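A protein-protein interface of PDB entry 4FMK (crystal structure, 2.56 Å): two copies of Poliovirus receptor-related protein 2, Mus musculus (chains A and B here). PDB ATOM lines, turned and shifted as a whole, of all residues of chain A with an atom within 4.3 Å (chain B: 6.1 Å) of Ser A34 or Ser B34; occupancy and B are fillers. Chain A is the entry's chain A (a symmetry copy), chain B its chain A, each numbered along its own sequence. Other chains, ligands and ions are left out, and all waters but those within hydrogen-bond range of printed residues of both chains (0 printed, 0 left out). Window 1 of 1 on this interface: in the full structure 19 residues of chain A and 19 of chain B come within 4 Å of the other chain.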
ATOM      1  N   ARG A  32     -33.040  -8.603  28.606  1.00  0.00           N
ATOM      2  CA  ARG A  32     -32.574  -9.653  27.742  1.00  0.00           C
ATOM      3  C   ARG A  32     -32.088 -10.834  28.566  1.00  0.00           C
ATOM      4  O   ARG A  32     -31.395 -10.669  29.551  1.00  0.00           O
ATOM      5  CB  ARG A  32     -31.390  -9.171  26.906  1.00  0.00           C
ATOM      6  CG  ARG A  32     -31.760  -8.589  25.576  1.00  0.00           C
ATOM      7  CD  ARG A  32     -31.197  -7.238  25.518  1.00  0.00           C
ATOM      8  NE  ARG A  32     -30.116  -7.135  24.557  1.00  0.00           N
ATOM      9  CZ  ARG A  32     -29.253  -6.105  24.490  1.00  0.00           C
ATOM     10  NH1 ARG A  32     -29.263  -5.101  25.395  1.00  0.00           N
ATOM     11  NH2 ARG A  32     -28.351  -6.100  23.523  1.00  0.00           N
ATOM     12  N   VAL A  33     -32.359 -12.039  28.096  1.00  0.00           N
ATOM     13  CA  VAL A  33     -32.108 -13.170  28.893  1.00  0.00           C
ATOM     14  C   VAL A  33     -30.832 -13.815  28.468  1.00  0.00           C
ATOM     15  O   VAL A  33     -30.652 -14.076  27.306  1.00  0.00           O
ATOM     16  CB  VAL A  33     -33.219 -14.182  28.756  1.00  0.00           C
ATOM     17  CG1 VAL A  33     -32.911 -15.399  29.635  1.00  0.00           C
ATOM     18  CG2 VAL A  33     -34.556 -13.517  29.052  1.00  0.00           C
ATOM     19  N   SER A  34     -29.932 -14.015  29.420  1.00  0.00           N
ATOM     20  CA  SER A  34     -28.578 -14.506  29.154  1.00  0.00           C
ATOM     21  C   SER A  34     -28.567 -15.975  29.370  1.00  0.00           C
ATOM     22  O   SER A  34     -27.714 -16.674  28.865  1.00  0.00           O
ATOM     23  CB  SER A  34     -27.602 -13.889  30.138  1.00  0.00           C
ATOM     24  OG  SER A  34     -27.569 -12.466  30.031  1.00  0.00           O
ATOM     25  N   GLN A  35     -29.489 -16.407  30.214  1.00  0.00           N
ATOM     26  CA  GLN A  35     -29.683 -17.823  30.547  1.00  0.00           C
ATOM     27  C   GLN A  35     -30.831 -18.011  31.528  1.00  0.00           C
ATOM     28  O   GLN A  35     -31.319 -17.060  32.097  1.00  0.00           O
ATOM     29  CB  GLN A  35     -28.405 -18.507  31.060  1.00  0.00           C
ATOM     30  CG  GLN A  35     -27.912 -18.111  32.443  1.00  0.00           C
ATOM     31  CD  GLN A  35     -26.777 -19.065  32.985  1.00  0.00           C
ATOM     32  OE1 GLN A  35     -25.761 -19.247  32.355  1.00  0.00           O
ATOM     33  NE2 GLN A  35     -26.969 -19.612  34.154  1.00  0.00           N
ATOM     34  N   HIS A  50     -29.435 -22.037  27.740  1.00  0.00           N
ATOM     35  CA  HIS A  50     -28.650 -20.900  27.232  1.00  0.00           C
ATOM     36  C   HIS A  50     -28.873 -20.680  25.736  1.00  0.00           C
ATOM     37  O   HIS A  50     -28.791 -21.643  24.948  1.00  0.00           O
ATOM     38  CB  HIS A  50     -27.159 -21.176  27.456  1.00  0.00           C
ATOM     39  CG  HIS A  50     -26.246 -20.036  27.083  1.00  0.00           C
ATOM     40  ND1 HIS A  50     -25.717 -19.211  28.000  1.00  0.00           N
ATOM     41  CD2 HIS A  50     -25.802 -19.588  25.855  1.00  0.00           C
ATOM     42  CE1 HIS A  50     -25.004 -18.247  27.375  1.00  0.00           C
ATOM     43  NE2 HIS A  50     -25.026 -18.502  26.069  1.00  0.00           N
ATOM     44  N   PRO A  51     -29.098 -19.429  25.312  1.00  0.00           N
ATOM     45  CA  PRO A  51     -29.430 -19.146  23.914  1.00  0.00           C
ATOM     46  C   PRO A  51     -28.430 -19.633  22.886  1.00  0.00           C
ATOM     47  O   PRO A  51     -28.783 -19.710  21.719  1.00  0.00           O
ATOM     48  CB  PRO A  51     -29.470 -17.590  23.840  1.00  0.00           C
ATOM     49  CG  PRO A  51     -29.517 -17.109  25.251  1.00  0.00           C
ATOM     50  CD  PRO A  51     -28.894 -18.189  26.101  1.00  0.00           C
ATOM     51  N   ALA A 103     -31.537 -15.255  34.295  1.00  0.00           N
ATOM     52  CA  ALA A 103     -30.471 -14.283  34.363  1.00  0.00           C
ATOM     53  C   ALA A 103     -30.639 -13.281  33.248  1.00  0.00           C
ATOM     54  O   ALA A 103     -30.360 -13.602  32.088  1.00  0.00           O
ATOM     55  CB  ALA A 103     -29.137 -14.952  34.258  1.00  0.00           C
ATOM     56  N   ARG B  32     -18.955 -21.749  31.792  1.00  0.00           N
ATOM     57  CA  ARG B  32     -18.960 -20.634  30.884  1.00  0.00           C
ATOM     58  C   ARG B  32     -19.807 -19.503  31.447  1.00  0.00           C
ATOM     59  O   ARG B  32     -20.889 -19.723  31.955  1.00  0.00           O
ATOM     60  CB  ARG B  32     -19.578 -21.036  29.548  1.00  0.00           C
ATOM     61  CG  ARG B  32     -18.596 -21.531  28.529  1.00  0.00           C
ATOM     62  CD  ARG B  32     -19.036 -22.865  28.111  1.00  0.00           C
ATOM     63  NE  ARG B  32     -19.509 -22.882  26.741  1.00  0.00           N
ATOM     64  CZ  ARG B  32     -20.211 -23.890  26.192  1.00  0.00           C
ATOM     65  NH1 ARG B  32     -20.626 -24.954  26.915  1.00  0.00           N
ATOM     66  NH2 ARG B  32     -20.527 -23.812  24.910  1.00  0.00           N
ATOM     67  N   VAL B  33     -19.363 -18.275  31.253  1.00  0.00           N
ATOM     68  CA  VAL B  33     -19.991 -17.196  31.901  1.00  0.00           C
ATOM     69  C   VAL B  33     -20.909 -16.501  30.954  1.00  0.00           C
ATOM     70  O   VAL B  33     -20.505 -16.157  29.873  1.00  0.00           O
ATOM     71  CB  VAL B  33     -18.972 -16.198  32.393  1.00  0.00           C
ATOM     72  CG1 VAL B  33     -19.691 -15.038  33.093  1.00  0.00           C
ATOM     73  CG2 VAL B  33     -17.937 -16.905  33.256  1.00  0.00           C
ATOM     74  N   SER B  34     -22.162 -16.350  31.358  1.00  0.00           N
ATOM     75  CA  SER B  34     -23.223 -15.818  30.501  1.00  0.00           C
ATOM     76  C   SER B  34     -23.365 -14.368  30.785  1.00  0.00           C
ATOM     77  O   SER B  34     -23.877 -13.620  29.977  1.00  0.00           O
ATOM     78  CB  SER B  34     -24.545 -16.484  30.839  1.00  0.00           C
ATOM     79  OG  SER B  34     -24.495 -17.896  30.631  1.00  0.00           O
ATOM     80  N   GLN B  35     -22.978 -14.012  31.998  1.00  0.00           N
ATOM     81  CA  GLN B  35     -22.997 -12.625  32.479  1.00  0.00           C
ATOM     82  C   GLN B  35     -22.476 -12.526  33.906  1.00  0.00           C
ATOM     83  O   GLN B  35     -22.310 -13.522  34.573  1.00  0.00           O
ATOM     84  CB  GLN B  35     -24.376 -11.955  32.350  1.00  0.00           C
ATOM     85  CG  GLN B  35     -25.472 -12.437  33.287  1.00  0.00           C
ATOM     86  CD  GLN B  35     -26.744 -11.503  33.272  1.00  0.00           C
ATOM     87  OE1 GLN B  35     -27.328 -11.259  32.240  1.00  0.00           O
ATOM     88  NE2 GLN B  35     -27.157 -11.041  34.421  1.00  0.00           N
ATOM     89  N   VAL B  36     -22.176 -11.313  34.327  1.00  0.00           N
ATOM     90  CA  VAL B  36     -21.726 -11.008  35.677  1.00  0.00           C
ATOM     91  C   VAL B  36     -22.414  -9.750  36.086  1.00  0.00           C
ATOM     92  O   VAL B  36     -22.463  -8.817  35.309  1.00  0.00           O
ATOM     93  CB  VAL B  36     -20.250 -10.636  35.746  1.00  0.00           C
ATOM     94  CG1 VAL B  36     -19.781 -10.759  37.179  1.00  0.00           C
ATOM     95  CG2 VAL B  36     -19.418 -11.533  34.864  1.00  0.00           C
ATOM     96  N   PHE B  49     -22.212  -6.815  33.421  1.00  0.00           N
ATOM     97  CA  PHE B  49     -21.368  -7.077  32.284  1.00  0.00           C
ATOM     98  C   PHE B  49     -21.816  -8.333  31.537  1.00  0.00           C
ATOM     99  O   PHE B  49     -21.992  -9.370  32.163  1.00  0.00           O
ATOM    100  CB  PHE B  49     -19.889  -7.242  32.692  1.00  0.00           C
ATOM    101  CG  PHE B  49     -19.057  -7.760  31.567  1.00  0.00           C
ATOM    102  CD1 PHE B  49     -18.726  -6.919  30.507  1.00  0.00           C
ATOM    103  CD2 PHE B  49     -18.794  -9.131  31.441  1.00  0.00           C
ATOM    104  CE1 PHE B  49     -18.038  -7.399  29.386  1.00  0.00           C
ATOM    105  CE2 PHE B  49     -18.105  -9.625  30.324  1.00  0.00           C
ATOM    106  CZ  PHE B  49     -17.731  -8.756  29.288  1.00  0.00           C
ATOM    107  N   HIS B  50     -21.921  -8.224  30.205  1.00  0.00           N
ATOM    108  CA  HIS B  50     -22.339  -9.310  29.303  1.00  0.00           C
ATOM    109  C   HIS B  50     -21.411  -9.430  28.093  1.00  0.00           C
ATOM    110  O   HIS B  50     -21.116  -8.414  27.434  1.00  0.00           O
ATOM    111  CB  HIS B  50     -23.754  -9.023  28.790  1.00  0.00           C
ATOM    112  CG  HIS B  50     -24.350 -10.118  27.943  1.00  0.00           C
ATOM    113  ND1 HIS B  50     -25.243 -10.995  28.426  1.00  0.00           N
ATOM    114  CD2 HIS B  50     -24.130 -10.473  26.626  1.00  0.00           C
ATOM    115  CE1 HIS B  50     -25.544 -11.901  27.467  1.00  0.00           C
ATOM    116  NE2 HIS B  50     -24.894 -11.557  26.359  1.00  0.00           N
ATOM    117  N   PRO B  51     -20.985 -10.654  27.747  1.00  0.00           N
ATOM    118  CA  PRO B  51     -20.010 -10.845  26.673  1.00  0.00           C
ATOM    119  C   PRO B  51     -20.391 -10.271  25.325  1.00  0.00           C
ATOM    120  O   PRO B  51     -19.515 -10.120  24.486  1.00  0.00           O
ATOM    121  CB  PRO B  51     -19.911 -12.393  26.521  1.00  0.00           C
ATOM    122  CG  PRO B  51     -20.549 -12.971  27.739  1.00  0.00           C
ATOM    123  CD  PRO B  51     -21.526 -11.941  28.250  1.00  0.00           C
ATOM    124  N   PHE B  53     -23.576  -7.902  24.999  1.00  0.00           N
ATOM    125  CA  PHE B  53     -24.334  -6.671  25.187  1.00  0.00           C
ATOM    126  C   PHE B  53     -23.460  -5.600  25.804  1.00  0.00           C
ATOM    127  O   PHE B  53     -23.841  -4.451  25.894  1.00  0.00           O
ATOM    128  CB  PHE B  53     -25.577  -6.929  26.059  1.00  0.00           C
ATOM    129  CG  PHE B  53     -26.433  -8.099  25.584  1.00  0.00           C
ATOM    130  CD1 PHE B  53     -26.721  -8.257  24.243  1.00  0.00           C
ATOM    131  CD2 PHE B  53     -26.950  -9.039  26.506  1.00  0.00           C
ATOM    132  CE1 PHE B  53     -27.510  -9.311  23.813  1.00  0.00           C
ATOM    133  CE2 PHE B  53     -27.732 -10.102  26.078  1.00  0.00           C
ATOM    134  CZ  PHE B  53     -28.004 -10.247  24.727  1.00  0.00           C
ATOM    135  N   LEU B  80     -13.228 -14.463  30.145  1.00  0.00           N
ATOM    136  CA  LEU B  80     -13.997 -13.435  30.978  1.00  0.00           C
ATOM    137  C   LEU B  80     -14.214 -13.589  32.504  1.00  0.00           C
ATOM    138  O   LEU B  80     -15.319 -13.442  33.010  1.00  0.00           O
ATOM    139  CB  LEU B  80     -15.326 -13.196  30.324  1.00  0.00           C
ATOM    140  CG  LEU B  80     -16.323 -12.280  31.010  1.00  0.00           C
ATOM    141  CD1 LEU B  80     -17.360 -13.150  31.683  1.00  0.00           C
ATOM    142  CD2 LEU B  80     -15.737 -11.257  31.983  1.00  0.00           C
ATOM    143  N   ALA B 103     -23.159 -15.478  36.470  1.00  0.00           N
ATOM    144  CA  ALA B 103     -24.106 -16.433  35.943  1.00  0.00           C
ATOM    145  C   ALA B 103     -23.397 -17.359  34.985  1.00  0.00           C
ATOM    146  O   ALA B 103     -23.082 -16.954  33.861  1.00  0.00           O
ATOM    147  CB  ALA B 103     -25.230 -15.734  35.247  1.00  0.00           C
ATOM    148  N   THR B 104     -23.204 -18.615  35.411  1.00  0.00           N
ATOM    149  CA  THR B 104     -22.556 -19.585  34.594  1.00  0.00           C
ATOM    150  C   THR B 104     -23.446 -20.771  34.153  1.00  0.00           C
ATOM    151  O   THR B 104     -24.483 -21.039  34.741  1.00  0.00           O
ATOM    152  CB  THR B 104     -21.326 -20.165  35.299  1.00  0.00           C
ATOM    153  OG1 THR B 104     -21.721 -21.224  36.139  1.00  0.00           O
ATOM    154  CG2 THR B 104     -20.687 -19.158  36.097  1.00  0.00           C
ATOM    155  N   PHE B 105     -22.944 -21.513  33.153  1.00  0.00           N
ATOM    156  CA  PHE B 105     -23.635 -22.612  32.503  1.00  0.00           C
ATOM    157  C   PHE B 105     -22.707 -23.787  32.491  1.00  0.00           C
ATOM    158  O   PHE B 105     -21.536 -23.675  32.112  1.00  0.00           O
ATOM    159  CB  PHE B 105     -23.953 -22.252  31.058  1.00  0.00           C
ATOM    160  CG  PHE B 105     -24.705 -23.292  30.300  1.00  0.00           C
ATOM    161  CD1 PHE B 105     -26.103 -23.309  30.312  1.00  0.00           C
ATOM    162  CD2 PHE B 105     -24.036 -24.193  29.471  1.00  0.00           C
ATOM    163  CE1 PHE B 105     -26.806 -24.180  29.542  1.00  0.00           C
ATOM    164  CE2 PHE B 105     -24.735 -25.120  28.721  1.00  0.00           C
ATOM    165  CZ  PHE B 105     -26.124 -25.108  28.748  1.00  0.00           C
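OG of Ser B34 sits at hydrogen-bond distance from OE1 of Gln A35 (2.5 Å).
OG of Ser B34 sits at hydrogen-bond distance from ND1 of His A50 (3.2 Å).
OG of Ser A34 lies within hydrogen-bond range of ND1 of His B50 (3.2 Å).
The side-chain hydroxyl (OG) of Ser A34 sits at hydrogen-bond distance from the side-chain amide oxygen (OE1) of Gln B35 (2.5 Å).
The backbone carbonyl oxygen (O) of Thr B104 is in hydrogen-bond range of the side-chain amide nitrogen (NE2) of Gln A35, 2.9 Å away.
The backbone NH of Phe B105 is in hydrogen-bond range of the backbone carbonyl oxygen of Arg B32, at 3.0 Å.
N of Ala A103 is in hydrogen-bond range of O of Gln A35, 2.9 Å away.
The backbone carbonyl oxygen (O) of Ser B34 lies within hydrogen-bond range of a ring nitrogen (ND1) of His B50 (3.3 Å).
The backbone NH of Ser A34 sits at hydrogen-bond distance from the backbone carbonyl oxygen of Ala A103.
The backbone NH (N) of Ala B103 lies within hydrogen-bond range of the backbone carbonyl oxygen (O) of Gln B35 (2.9 Å).
The backbone NH (N) of Ser B34 sits at hydrogen-bond distance from the backbone carbonyl oxygen (O) of Ala B103.
Among the printed residues, pairs that only touch across the chains: Arg A32 with Phe B53 (2.8 Å), His A50 with Phe B105 (3.7 Å), Gln A35 with Phe B105 (3.7 Å), Ser A34 with Ser B34 (3.7 Å), Gln A35 with Ala B103 (3.8 Å) and Ala A103 with Gln B35 (3.8 Å).
Ser A34 touches just these residues of chain B: Ser B34, Gln B35 and His B50.
Phe B49 touches none of the printed residues of chain A.
Of the printed residues of chain A, His B50 touches Ser A34.
Printed residues of chain A within 4 Å of Ala B103: Gln A35 (3.8 Å).
The nearest residue of chain B that does not touch Ser A34 is Phe B53 (4.6 Å).
The nearest printed residue of chain A that does not touch Ala B103 is Ala A103 (4.1 Å).
Of the 13 printed residues of chain B, 7 touch a printed residue of chain A.
Hydrophobic or aromatic side chains of chain B within 4 Å of the printed part of chain A: His B50, Phe B53 and Phe B105.
Along chain B the printed residues that touch a printed residue of chain A span positions 34 to 105.
Ser B34 touches its own counterpart, Ser A34.
Ser A34 touches Gln B35, and with the chains exchanged Gln A35 touches Ser B34.
Ser A34 touches His B50, and with the chains exchanged His A50 touches Ser B34.
Gln A35 touches Ala B103, and with the chains exchanged Ala A103 touches Gln B35.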
